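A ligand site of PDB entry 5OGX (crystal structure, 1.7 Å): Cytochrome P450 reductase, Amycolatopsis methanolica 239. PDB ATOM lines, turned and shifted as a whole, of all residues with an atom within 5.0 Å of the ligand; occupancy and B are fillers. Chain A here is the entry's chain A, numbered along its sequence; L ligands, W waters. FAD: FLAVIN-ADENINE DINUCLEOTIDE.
The backbone NH (N) of Thr 174 lies within hydrogen-bond range of an oxygen (O2P) of the ligand, 2.9 Å away. OG1 of Thr 174 lies within hydrogen-bond range of O2P of the ligand (2.6 Å). An oxygen (O2') of the ligand sits at hydrogen-bond distance from the backbone NH (N) of Gln 148 (3.2 Å). An oxygen (O2') of the ligand lies within hydrogen-bond range of the backbone carbonyl oxygen (O) of Gln 148 (2.6 Å). An oxygen (O2') of the ligand is in hydrogen-bond range of the side-chain amide oxygen of Gln 148 (3.2 Å). The chain-end carboxylate (O) of Ser 336 is in hydrogen-bond range of an oxygen (O2B) of the ligand, at 2.7 Å. OG of Ser 336 lies within hydrogen-bond range of O2A of the ligand. The backbone carbonyl oxygen (O) of His 164 is in hydrogen-bond range of a nitrogen (N3) of the ligand, 2.7 Å away. The backbone NH (N) of Ala 173 is in hydrogen-bond range of an oxygen (O1P) of the ligand. O2 of the ligand lies within hydrogen-bond range of N of Arg 166 (2.9 Å). The side-chain hydroxyl (OH) of Tyr 149 sits at hydrogen-bond distance from an oxygen (O4') of the ligand, 2.9 Å away. The backbone NH (N) of Val 172 is in hydrogen-bond range of an oxygen (O1A) of the ligand, 2.9 Å away. The guanidinium group (NE) of Arg 147 lies within salt-bridge range of an oxygen (O1P) of the ligand (2.9 Å). O4 of the ligand is in hydrogen-bond range of N of Ser 150 (3.0 Å). N5 of the ligand lies within hydrogen-bond range of OG of Ser 150, at 3.3 Å. The side-chain hydroxyl of Thr 217 is in hydrogen-bond range of an oxygen (O2) of the ligand.
Water W4 lies within hydrogen-bond range of O1A of the ligand and OG of Ser 336. Water W9 lies within hydrogen-bond range of O3' of the ligand, O of Thr 333, OE1 of Gln 148 and N of Ala 335. Water W7 lies within hydrogen-bond range of O2A of the ligand and N of Ala 335. Water W6 lies within hydrogen-bond range of OXT of Ser 336 (2.7 Å) and O3B of the ligand (2.8 Å). Water W5 bridges the backbone carbonyl oxygen of Phe 332 and a nitrogen (N6A) of the ligand. Water W1 bridges O of Gly 170 (2.4 Å) and O1A of the ligand (3.3 Å).
OG1 of Thr 174 lies within hydrogen-bond range of N of Val 168 (3.0 Å). The side-chain amide oxygen (OE1) of Gln 39 sits at hydrogen-bond distance from the side-chain amide nitrogen (NE2) of Gln 148 (3.0 Å). NE2 of Gln 148 lies within hydrogen-bond range of O of Cys 37. O of Pro 334 sits at hydrogen-bond distance from NE2 of Gln 39 (3.3 Å). The backbone carbonyl oxygen of Cys 37 sits close to the side-chain hydroxyl of Tyr 135 (3.2 Å). O of Thr 333 lies within hydrogen-bond range of NE2 of Gln 39 (3.1 Å).
Residues that only touch the ligand: Ser 36 (3.8 Å), Tyr 135 (3.7 Å), Val 165 (3.5 Å), Val 168 (3.6 Å), Gly 171 (3.3 Å), Lys 331 (3.6 Å), Phe 332 (3.1 Å), Thr 333 (3.8 Å) and Pro 334 (3.5 Å). Hydrophobic or aromatic side chains within 4 Å of the ligand: Tyr 135, Tyr 149, Val 168, Val 172, Ala 173, Phe 332 and Pro 334. 20 residues have an atom within 4 Å of the ligand: Ser 36, Tyr 135, Arg 147, Gln 148, Tyr 149, Ser 150, His 164, Val 165, Arg 166, Val 168, Gly 171, Val 172, Ala 173, Thr 174, Thr 217, Lys 331, Phe 332, Thr 333, Pro 334 and Ser 336.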
ATOM      1  N   SER A  36       9.550 -17.819  30.837  1.00  0.00           N
ATOM      2  CA  SER A  36       9.776 -17.333  29.479  1.00  0.00           C
ATOM      3  C   SER A  36      11.244 -17.014  29.197  1.00  0.00           C
ATOM      4  O   SER A  36      11.509 -16.305  28.218  1.00  0.00           O
ATOM      5  CB  SER A  36       9.003 -16.027  29.195  1.00  0.00           C
ATOM      6  OG  SER A  36       7.640 -16.246  28.874  1.00  0.00           O
ATOM      7  N   CYS A  37      12.190 -17.476  30.025  1.00  0.00           N
ATOM      8  CA  CYS A  37      13.606 -17.224  29.759  1.00  0.00           C
ATOM      9  C   CYS A  37      14.536 -18.131  30.557  1.00  0.00           C
ATOM     10  O   CYS A  37      15.656 -18.413  30.120  1.00  0.00           O
ATOM     11  CB  CYS A  37      13.961 -15.746  30.012  1.00  0.00           C
ATOM     12  SG  CYS A  37      14.202 -15.319  31.765  1.00  0.00           S
ATOM     13  N   GLN A  39      16.333 -17.420  32.902  1.00  0.00           N
ATOM     14  CA  GLN A  39      17.597 -16.747  33.165  1.00  0.00           C
ATOM     15  C   GLN A  39      17.430 -15.461  33.975  1.00  0.00           C
ATOM     16  O   GLN A  39      18.387 -14.685  34.072  1.00  0.00           O
ATOM     17  CB  GLN A  39      18.340 -16.441  31.838  1.00  0.00           C
ATOM     18  CG  GLN A  39      17.679 -15.343  31.018  1.00  0.00           C
ATOM     19  CD  GLN A  39      18.459 -14.980  29.757  1.00  0.00           C
ATOM     20  OE1 GLN A  39      19.347 -15.718  29.324  1.00  0.00           O
ATOM     21  NE2 GLN A  39      18.129 -13.830  29.165  1.00  0.00           N
ATOM     22  N   TYR A 135      10.732 -23.540  23.434  1.00  0.00           N
ATOM     23  CA  TYR A 135      12.142 -23.469  23.089  1.00  0.00           C
ATOM     24  C   TYR A 135      12.917 -24.527  23.848  1.00  0.00           C
ATOM     25  O   TYR A 135      12.401 -25.178  24.761  1.00  0.00           O
ATOM     26  CB  TYR A 135      12.701 -22.052  23.347  1.00  0.00           C
ATOM     27  CG  TYR A 135      12.961 -21.690  24.816  1.00  0.00           C
ATOM     28  CD1 TYR A 135      14.167 -21.995  25.424  1.00  0.00           C
ATOM     29  CD2 TYR A 135      12.015 -20.991  25.564  1.00  0.00           C
ATOM     30  CE1 TYR A 135      14.424 -21.654  26.754  1.00  0.00           C
ATOM     31  CE2 TYR A 135      12.266 -20.639  26.913  1.00  0.00           C
ATOM     32  CZ  TYR A 135      13.484 -20.967  27.473  1.00  0.00           C
ATOM     33  OH  TYR A 135      13.760 -20.637  28.815  1.00  0.00           O
ATOM     34  N   ARG A 147      22.114 -21.187  26.509  1.00  0.00           N
ATOM     35  CA  ARG A 147      21.442 -20.305  25.562  1.00  0.00           C
ATOM     36  C   ARG A 147      20.175 -20.968  25.046  1.00  0.00           C
ATOM     37  O   ARG A 147      20.125 -22.193  24.876  1.00  0.00           O
ATOM     38  CB  ARG A 147      22.350 -19.932  24.385  1.00  0.00           C
ATOM     39  CG  ARG A 147      23.652 -19.236  24.808  1.00  0.00           C
ATOM     40  CD  ARG A 147      23.400 -17.831  25.329  1.00  0.00           C
ATOM     41  NE  ARG A 147      24.661 -17.102  25.494  1.00  0.00           N
ATOM     42  CZ  ARG A 147      25.331 -17.015  26.639  1.00  0.00           C
ATOM     43  NH1 ARG A 147      24.872 -17.615  27.739  1.00  0.00           N
ATOM     44  NH2 ARG A 147      26.475 -16.331  26.684  1.00  0.00           N
ATOM     45  N   GLN A 148      19.153 -20.144  24.828  1.00  0.00           N
ATOM     46  CA  GLN A 148      17.828 -20.579  24.414  1.00  0.00           C
ATOM     47  C   GLN A 148      17.694 -20.487  22.897  1.00  0.00           C
ATOM     48  O   GLN A 148      18.082 -19.465  22.308  1.00  0.00           O
ATOM     49  CB  GLN A 148      16.774 -19.678  25.053  1.00  0.00           C
ATOM     50  CG  GLN A 148      16.917 -19.503  26.559  1.00  0.00           C
ATOM     51  CD  GLN A 148      17.815 -18.332  27.011  1.00  0.00           C
ATOM     52  OE1 GLN A 148      18.700 -17.863  26.276  1.00  0.00           O
ATOM     53  NE2 GLN A 148      17.591 -17.872  28.228  1.00  0.00           N
ATOM     54  N   TYR A 149      17.047 -21.484  22.293  1.00  0.00           N
ATOM     55  CA  TYR A 149      16.736 -21.443  20.865  1.00  0.00           C
ATOM     56  C   TYR A 149      15.329 -21.961  20.659  1.00  0.00           C
ATOM     57  O   TYR A 149      14.989 -23.067  21.108  1.00  0.00           O
ATOM     58  CB  TYR A 149      17.767 -22.244  20.033  1.00  0.00           C
ATOM     59  CG  TYR A 149      19.081 -21.527  20.131  1.00  0.00           C
ATOM     60  CD1 TYR A 149      19.282 -20.325  19.464  1.00  0.00           C
ATOM     61  CD2 TYR A 149      20.062 -21.948  21.015  1.00  0.00           C
ATOM     62  CE1 TYR A 149      20.469 -19.611  19.608  1.00  0.00           C
ATOM     63  CE2 TYR A 149      21.245 -21.246  21.171  1.00  0.00           C
ATOM     64  CZ  TYR A 149      21.441 -20.074  20.487  1.00  0.00           C
ATOM     65  OH  TYR A 149      22.605 -19.359  20.660  1.00  0.00           O
ATOM     66  N   SER A 150      14.499 -21.147  20.017  1.00  0.00           N
ATOM     67  CA  SER A 150      13.107 -21.503  19.782  1.00  0.00           C
ATOM     68  C   SER A 150      12.985 -22.641  18.782  1.00  0.00           C
ATOM     69  O   SER A 150      13.764 -22.748  17.828  1.00  0.00           O
ATOM     70  CB  SER A 150      12.352 -20.299  19.208  1.00  0.00           C
ATOM     71  OG  SER A 150      12.378 -19.202  20.088  1.00  0.00           O
ATOM     72  N   HIS A 164      16.590 -21.931  14.246  1.00  0.00           N
ATOM     73  CA  HIS A 164      17.086 -20.872  13.355  1.00  0.00           C
ATOM     74  C   HIS A 164      17.973 -19.963  14.190  1.00  0.00           C
ATOM     75  O   HIS A 164      17.489 -19.294  15.100  1.00  0.00           O
ATOM     76  CB  HIS A 164      15.953 -20.044  12.740  1.00  0.00           C
ATOM     77  CG  HIS A 164      14.941 -20.863  12.000  1.00  0.00           C
ATOM     78  ND1 HIS A 164      13.774 -20.313  11.517  1.00  0.00           N
ATOM     79  CD2 HIS A 164      14.927 -22.175  11.650  1.00  0.00           C
ATOM     80  CE1 HIS A 164      13.074 -21.262  10.905  1.00  0.00           C
ATOM     81  NE2 HIS A 164      13.749 -22.388  10.963  1.00  0.00           N
ATOM     82  N   VAL A 165      19.268 -19.916  13.863  1.00  0.00           N
ATOM     83  CA  VAL A 165      20.263 -19.272  14.703  1.00  0.00           C
ATOM     84  C   VAL A 165      20.839 -18.068  13.970  1.00  0.00           C
ATOM     85  O   VAL A 165      21.355 -18.196  12.867  1.00  0.00           O
ATOM     86  CB  VAL A 165      21.387 -20.246  15.084  1.00  0.00           C
ATOM     87  CG1 VAL A 165      22.345 -19.593  16.073  1.00  0.00           C
ATOM     88  CG2 VAL A 165      20.790 -21.519  15.673  1.00  0.00           C
ATOM     89  N   ARG A 166      20.788 -16.899  14.617  1.00  0.00           N
ATOM     90  CA  ARG A 166      21.417 -15.693  14.087  1.00  0.00           C
ATOM     91  C   ARG A 166      22.797 -15.503  14.713  1.00  0.00           C
ATOM     92  O   ARG A 166      22.933 -15.577  15.936  1.00  0.00           O
ATOM     93  CB  ARG A 166      20.539 -14.472  14.342  1.00  0.00           C
ATOM     94  CG  ARG A 166      21.174 -13.179  13.892  1.00  0.00           C
ATOM     95  CD  ARG A 166      20.717 -12.773  12.497  1.00  0.00           C
ATOM     96  NE  ARG A 166      21.336 -11.506  12.100  1.00  0.00           N
ATOM     97  CZ  ARG A 166      20.942 -10.312  12.529  1.00  0.00           C
ATOM     98  NH1 ARG A 166      21.575  -9.219  12.103  1.00  0.00           N
ATOM     99  NH2 ARG A 166      19.923 -10.207  13.363  1.00  0.00           N
ATOM    100  N   VAL A 168      25.735 -13.700  16.290  1.00  0.00           N
ATOM    101  CA  VAL A 168      26.008 -12.477  17.044  1.00  0.00           C
ATOM    102  C   VAL A 168      27.530 -12.283  17.071  1.00  0.00           C
ATOM    103  O   VAL A 168      28.242 -13.142  17.583  1.00  0.00           O
ATOM    104  CB  VAL A 168      25.433 -12.555  18.471  1.00  0.00           C
ATOM    105  CG1 VAL A 168      25.859 -11.348  19.273  1.00  0.00           C
ATOM    106  CG2 VAL A 168      23.900 -12.677  18.415  1.00  0.00           C
ATOM    107  N   PRO A 169      28.047 -11.201  16.501  1.00  0.00           N
ATOM    108  CA  PRO A 169      29.503 -10.979  16.512  1.00  0.00           C
ATOM    109  C   PRO A 169      30.076 -11.023  17.920  1.00  0.00           C
ATOM    110  O   PRO A 169      29.563 -10.382  18.842  1.00  0.00           O
ATOM    111  CB  PRO A 169      29.649  -9.593  15.881  1.00  0.00           C
ATOM    112  CG  PRO A 169      28.482  -9.500  14.947  1.00  0.00           C
ATOM    113  CD  PRO A 169      27.351 -10.198  15.670  1.00  0.00           C
ATOM    114  N   GLY A 170      31.141 -11.803  18.084  1.00  0.00           N
ATOM    115  CA  GLY A 170      31.754 -11.993  19.380  1.00  0.00           C
ATOM    116  C   GLY A 170      30.971 -12.855  20.337  1.00  0.00           C
ATOM    117  O   GLY A 170      31.348 -12.939  21.500  1.00  0.00           O
ATOM    118  N   GLY A 171      29.898 -13.505  19.877  1.00  0.00           N
ATOM    119  CA  GLY A 171      29.050 -14.286  20.772  1.00  0.00           C
ATOM    120  C   GLY A 171      29.663 -15.636  21.126  1.00  0.00           C
ATOM    121  O   GLY A 171      30.336 -16.278  20.321  1.00  0.00           O
ATOM    122  N   VAL A 172      29.416 -16.058  22.365  1.00  0.00           N
ATOM    123  CA  VAL A 172      29.976 -17.314  22.857  1.00  0.00           C
ATOM    124  C   VAL A 172      29.340 -18.502  22.125  1.00  0.00           C
ATOM    125  O   VAL A 172      30.050 -19.376  21.621  1.00  0.00           O
ATOM    126  CB  VAL A 172      29.791 -17.405  24.382  1.00  0.00           C
ATOM    127  CG1 VAL A 172      30.052 -18.825  24.891  1.00  0.00           C
ATOM    128  CG2 VAL A 172      30.714 -16.412  25.067  1.00  0.00           C
ATOM    129  N   ALA A 173      28.000 -18.538  22.066  1.00  0.00           N
ATOM    130  CA  ALA A 173      27.334 -19.691  21.460  1.00  0.00           C
ATOM    131  C   ALA A 173      27.314 -19.611  19.938  1.00  0.00           C
ATOM    132  O   ALA A 173      27.419 -20.640  19.277  1.00  0.00           O
ATOM    133  CB  ALA A 173      25.899 -19.825  21.973  1.00  0.00           C
ATOM    134  N   THR A 174      27.130 -18.413  19.367  1.00  0.00           N
ATOM    135  CA  THR A 174      26.932 -18.327  17.918  1.00  0.00           C
ATOM    136  C   THR A 174      28.273 -18.186  17.209  1.00  0.00           C
ATOM    137  O   THR A 174      28.752 -19.150  16.596  1.00  0.00           O
ATOM    138  CB  THR A 174      25.957 -17.192  17.585  1.00  0.00           C
ATOM    139  OG1 THR A 174      26.450 -15.955  18.125  1.00  0.00           O
ATOM    140  CG2 THR A 174      24.610 -17.497  18.183  1.00  0.00           C
ATOM    141  N   ASP A 175      28.892 -17.005  17.296  1.00  0.00           N
ATOM    142  CA  ASP A 175      30.194 -16.779  16.686  1.00  0.00           C
ATOM    143  C   ASP A 175      31.216 -17.833  17.122  1.00  0.00           C
ATOM    144  O   ASP A 175      32.051 -18.265  16.319  1.00  0.00           O
ATOM    145  CB  ASP A 175      30.684 -15.377  17.055  1.00  0.00           C
ATOM    146  CG  ASP A 175      31.319 -14.629  15.883  1.00  0.00           C
ATOM    147  OD1 ASP A 175      31.164 -15.048  14.717  1.00  0.00           O
ATOM    148  OD2 ASP A 175      31.961 -13.587  16.149  1.00  0.00           O
ATOM    149  N   THR A 217      15.768 -13.905  13.533  1.00  0.00           N
ATOM    150  CA  THR A 217      15.408 -15.291  13.782  1.00  0.00           C
ATOM    151  C   THR A 217      14.265 -15.431  14.792  1.00  0.00           C
ATOM    152  O   THR A 217      13.892 -16.566  15.102  1.00  0.00           O
ATOM    153  CB  THR A 217      16.614 -16.094  14.247  1.00  0.00           C
ATOM    154  OG1 THR A 217      17.297 -15.338  15.253  1.00  0.00           O
ATOM    155  CG2 THR A 217      17.574 -16.368  13.067  1.00  0.00           C
ATOM    156  N   ALA A 220      11.485 -17.947  14.041  1.00  0.00           N
ATOM    157  CA  ALA A 220      11.470 -19.395  14.240  1.00  0.00           C
ATOM    158  C   ALA A 220      10.218 -19.922  14.948  1.00  0.00           C
ATOM    159  O   ALA A 220       9.539 -20.790  14.389  1.00  0.00           O
ATOM    160  CB  ALA A 220      12.728 -19.850  14.988  1.00  0.00           C
ATOM    161  N   GLU A 330       7.563 -13.138  23.065  1.00  0.00           N
ATOM    162  CA  GLU A 330       8.754 -13.925  23.366  1.00  0.00           C
ATOM    163  C   GLU A 330       9.976 -13.044  23.109  1.00  0.00           C
ATOM    164  O   GLU A 330      10.278 -12.705  21.962  1.00  0.00           O
ATOM    165  CB  GLU A 330       8.828 -15.215  22.523  1.00  0.00           C
ATOM    166  CG  GLU A 330       9.994 -16.125  22.917  1.00  0.00           C
ATOM    167  CD  GLU A 330       9.623 -17.029  24.087  1.00  0.00           C
ATOM    168  OE1 GLU A 330       9.207 -16.499  25.137  1.00  0.00           O
ATOM    169  OE2 GLU A 330       9.721 -18.263  23.944  1.00  0.00           O
ATOM    170  N   LYS A 331      10.695 -12.664  24.161  1.00  0.00           N
ATOM    171  CA  LYS A 331      11.838 -11.786  23.972  1.00  0.00           C
ATOM    172  C   LYS A 331      13.146 -12.567  23.974  1.00  0.00           C
ATOM    173  O   LYS A 331      13.414 -13.336  24.911  1.00  0.00           O
ATOM    174  CB  LYS A 331      11.883 -10.709  25.056  1.00  0.00           C
ATOM    175  CG  LYS A 331      10.552 -10.012  25.244  1.00  0.00           C
ATOM    176  CD  LYS A 331      10.612  -9.119  26.472  1.00  0.00           C
ATOM    177  CE  LYS A 331       9.661  -7.973  26.360  1.00  0.00           C
ATOM    178  NZ  LYS A 331       9.270  -7.502  27.720  1.00  0.00           N
ATOM    179  N   PHE A 332      13.955 -12.370  22.924  1.00  0.00           N
ATOM    180  CA  PHE A 332      15.280 -12.979  22.796  1.00  0.00           C
ATOM    181  C   PHE A 332      16.284 -12.146  23.584  1.00  0.00           C
ATOM    182  O   PHE A 332      17.211 -11.527  23.044  1.00  0.00           O
ATOM    183  CB  PHE A 332      15.695 -13.080  21.323  1.00  0.00           C
ATOM    184  CG  PHE A 332      14.947 -14.134  20.521  1.00  0.00           C
ATOM    185  CD1 PHE A 332      13.957 -14.897  21.085  1.00  0.00           C
ATOM    186  CD2 PHE A 332      15.282 -14.363  19.180  1.00  0.00           C
ATOM    187  CE1 PHE A 332      13.281 -15.871  20.357  1.00  0.00           C
ATOM    188  CE2 PHE A 332      14.623 -15.330  18.431  1.00  0.00           C
ATOM    189  CZ  PHE A 332      13.618 -16.086  19.025  1.00  0.00           C
ATOM    190  N   THR A 333      16.107 -12.130  24.906  1.00  0.00           N
ATOM    191  CA  THR A 333      16.942 -11.289  25.747  1.00  0.00           C
ATOM    192  C   THR A 333      18.355 -11.855  25.859  1.00  0.00           C
ATOM    193  O   THR A 333      18.506 -13.034  26.205  1.00  0.00           O
ATOM    194  CB  THR A 333      16.332 -11.145  27.126  1.00  0.00           C
ATOM    195  OG1 THR A 333      15.025 -10.560  27.006  1.00  0.00           O
ATOM    196  CG2 THR A 333      17.193 -10.250  27.982  1.00  0.00           C
ATOM    197  N   PRO A 334      19.394 -11.078  25.597  1.00  0.00           N
ATOM    198  CA  PRO A 334      20.753 -11.577  25.749  1.00  0.00           C
ATOM    199  C   PRO A 334      21.002 -12.139  27.145  1.00  0.00           C
ATOM    200  O   PRO A 334      20.454 -11.666  28.136  1.00  0.00           O
ATOM    201  CB  PRO A 334      21.619 -10.338  25.487  1.00  0.00           C
ATOM    202  CG  PRO A 334      20.792  -9.547  24.505  1.00  0.00           C
ATOM    203  CD  PRO A 334      19.371  -9.724  24.993  1.00  0.00           C
ATOM    204  N   ALA A 335      21.844 -13.174  27.189  1.00  0.00           N
ATOM    205  CA  ALA A 335      22.205 -13.867  28.413  1.00  0.00           C
ATOM    206  C   ALA A 335      23.488 -13.337  29.016  1.00  0.00           C
ATOM    207  O   ALA A 335      23.911 -13.839  30.059  1.00  0.00           O
ATOM    208  CB  ALA A 335      22.361 -15.371  28.133  1.00  0.00           C
ATOM    209  N   SER A 336      24.122 -12.370  28.373  1.00  0.00           N
ATOM    210  CA  SER A 336      25.371 -11.793  28.869  1.00  0.00           C
ATOM    211  C   SER A 336      25.503 -10.358  28.393  1.00  0.00           C
ATOM    212  O   SER A 336      24.654  -9.856  27.656  1.00  0.00           O
ATOM    213  CB  SER A 336      26.575 -12.623  28.399  1.00  0.00           C
ATOM    214  OG  SER A 336      26.787 -12.472  27.009  1.00  0.00           O
ATOM    215  OXT SER A 336      26.462  -9.664  28.742  1.00  0.00           O
HETATM  216  PA  FAD L   1      26.699 -13.670  23.851  1.00  0.00           P
HETATM  217  O1A FAD L   1      28.102 -14.177  24.087  1.00  0.00           O
HETATM  218  O2A FAD L   1      25.754 -13.928  24.993  1.00  0.00           O
HETATM  219  O5B FAD L   1      26.716 -12.042  23.560  1.00  0.00           O
HETATM  220  C5B FAD L   1      27.855 -11.461  22.982  1.00  0.00           C
HETATM  221  C4B FAD L   1      27.698  -9.909  23.106  1.00  0.00           C
HETATM  222  O4B FAD L   1      26.776  -9.504  22.267  1.00  0.00           O
HETATM  223  C3B FAD L   1      27.181  -9.537  24.503  1.00  0.00           C
HETATM  224  O3B FAD L   1      27.749  -8.371  24.883  1.00  0.00           O
HETATM  225  C2B FAD L   1      25.645  -9.417  24.318  1.00  0.00           C
HETATM  226  O2B FAD L   1      25.032  -8.536  25.359  1.00  0.00           O
HETATM  227  C1B FAD L   1      25.517  -8.942  23.108  1.00  0.00           C
HETATM  228  N9A FAD L   1      24.373  -9.492  22.422  1.00  0.00           N
HETATM  229  C8A FAD L   1      23.713 -10.604  22.749  1.00  0.00           C
HETATM  230  N7A FAD L   1      22.731 -10.782  21.854  1.00  0.00           N
HETATM  231  C5A FAD L   1      22.804  -9.764  20.972  1.00  0.00           C
HETATM  232  C6A FAD L   1      22.044  -9.463  19.859  1.00  0.00           C
HETATM  233  N6A FAD L   1      20.901 -10.014  19.153  1.00  0.00           N
HETATM  234  N1A FAD L   1      22.322  -8.386  19.138  1.00  0.00           N
HETATM  235  C2A FAD L   1      23.355  -7.586  19.488  1.00  0.00           C
HETATM  236  N3A FAD L   1      24.106  -7.872  20.579  1.00  0.00           N
HETATM  237  C4A FAD L   1      23.820  -8.975  21.312  1.00  0.00           C
HETATM  238  N1  FAD L   1      18.529 -16.571  19.195  1.00  0.00           N
HETATM  239  C2  FAD L   1      18.424 -17.117  17.844  1.00  0.00           C
HETATM  240  O2  FAD L   1      19.252 -16.862  17.031  1.00  0.00           O
HETATM  241  N3  FAD L   1      17.299 -17.997  17.510  1.00  0.00           N
HETATM  242  C4  FAD L   1      16.264 -18.330  18.446  1.00  0.00           C
HETATM  243  O4  FAD L   1      15.365 -19.041  18.131  1.00  0.00           O
HETATM  244  C4X FAD L   1      16.387 -17.736  19.811  1.00  0.00           C
HETATM  245  N5  FAD L   1      15.392 -18.074  20.779  1.00  0.00           N
HETATM  246  C5X FAD L   1      15.519 -17.471  22.104  1.00  0.00           C
HETATM  247  C6  FAD L   1      14.510 -17.752  23.034  1.00  0.00           C
HETATM  248  C7  FAD L   1      14.650 -17.172  24.302  1.00  0.00           C
HETATM  249  C7M FAD L   1      13.482 -17.596  25.192  1.00  0.00           C
HETATM  250  C8  FAD L   1      15.732 -16.356  24.622  1.00  0.00           C
HETATM  251  C8M FAD L   1      15.796 -15.781  26.028  1.00  0.00           C
HETATM  252  C9  FAD L   1      16.719 -16.079  23.681  1.00  0.00           C
HETATM  253  C9A FAD L   1      16.598 -16.632  22.431  1.00  0.00           C
HETATM  254  N10 FAD L   1      17.656 -16.339  21.451  1.00  0.00           N
HETATM  255  C10 FAD L   1      17.510 -16.892  20.140  1.00  0.00           C
HETATM  256  C1' FAD L   1      18.836 -15.527  21.805  1.00  0.00           C
HETATM  257  C2' FAD L   1      19.927 -16.643  22.090  1.00  0.00           C
HETATM  258  O2' FAD L   1      19.610 -17.488  23.184  1.00  0.00           O
HETATM  259  C3' FAD L   1      21.338 -16.091  22.363  1.00  0.00           C
HETATM  260  O3' FAD L   1      21.230 -15.059  23.305  1.00  0.00           O
HETATM  261  C4' FAD L   1      21.988 -15.540  21.074  1.00  0.00           C
HETATM  262  O4' FAD L   1      22.168 -16.572  20.144  1.00  0.00           O
HETATM  263  C5' FAD L   1      23.358 -14.902  21.376  1.00  0.00           C
HETATM  264  O5' FAD L   1      24.112 -15.773  22.203  1.00  0.00           O
HETATM  265  P   FAD L   1      25.750 -15.751  22.094  1.00  0.00           P
HETATM  266  O1P FAD L   1      26.273 -16.674  23.160  1.00  0.00           O
HETATM  267  O2P FAD L   1      26.205 -16.044  20.685  1.00  0.00           O
HETATM  268  O3P FAD L   1      26.159 -14.205  22.412  1.00  0.00           O
HETATM  269  O   HOH W   1      31.190 -13.101  23.911  1.00  0.00           O
HETATM  270  O   HOH W   2      21.270 -15.495  17.887  1.00  0.00           O
HETATM  271  O   HOH W   3      20.547 -12.595  22.122  1.00  0.00           O
HETATM  272  O   HOH W   4      29.553 -13.096  25.882  1.00  0.00           O
HETATM  273  O   HOH W   5      18.454 -10.838  20.917  1.00  0.00           O
HETATM  274  O   HOH W   6      27.140  -7.414  27.447  1.00  0.00           O
HETATM  275  O   HOH W   7      23.144 -13.555  24.665  1.00  0.00           O
HETATM  276  O   HOH W   8      15.726 -21.417  16.762  1.00  0.00           O
HETATM  277  O   HOH W   9      19.870 -15.370  25.505  1.00  0.00           O
HETATM  278  O   HOH W  10      20.288 -13.018  18.887  1.00  0.00           O
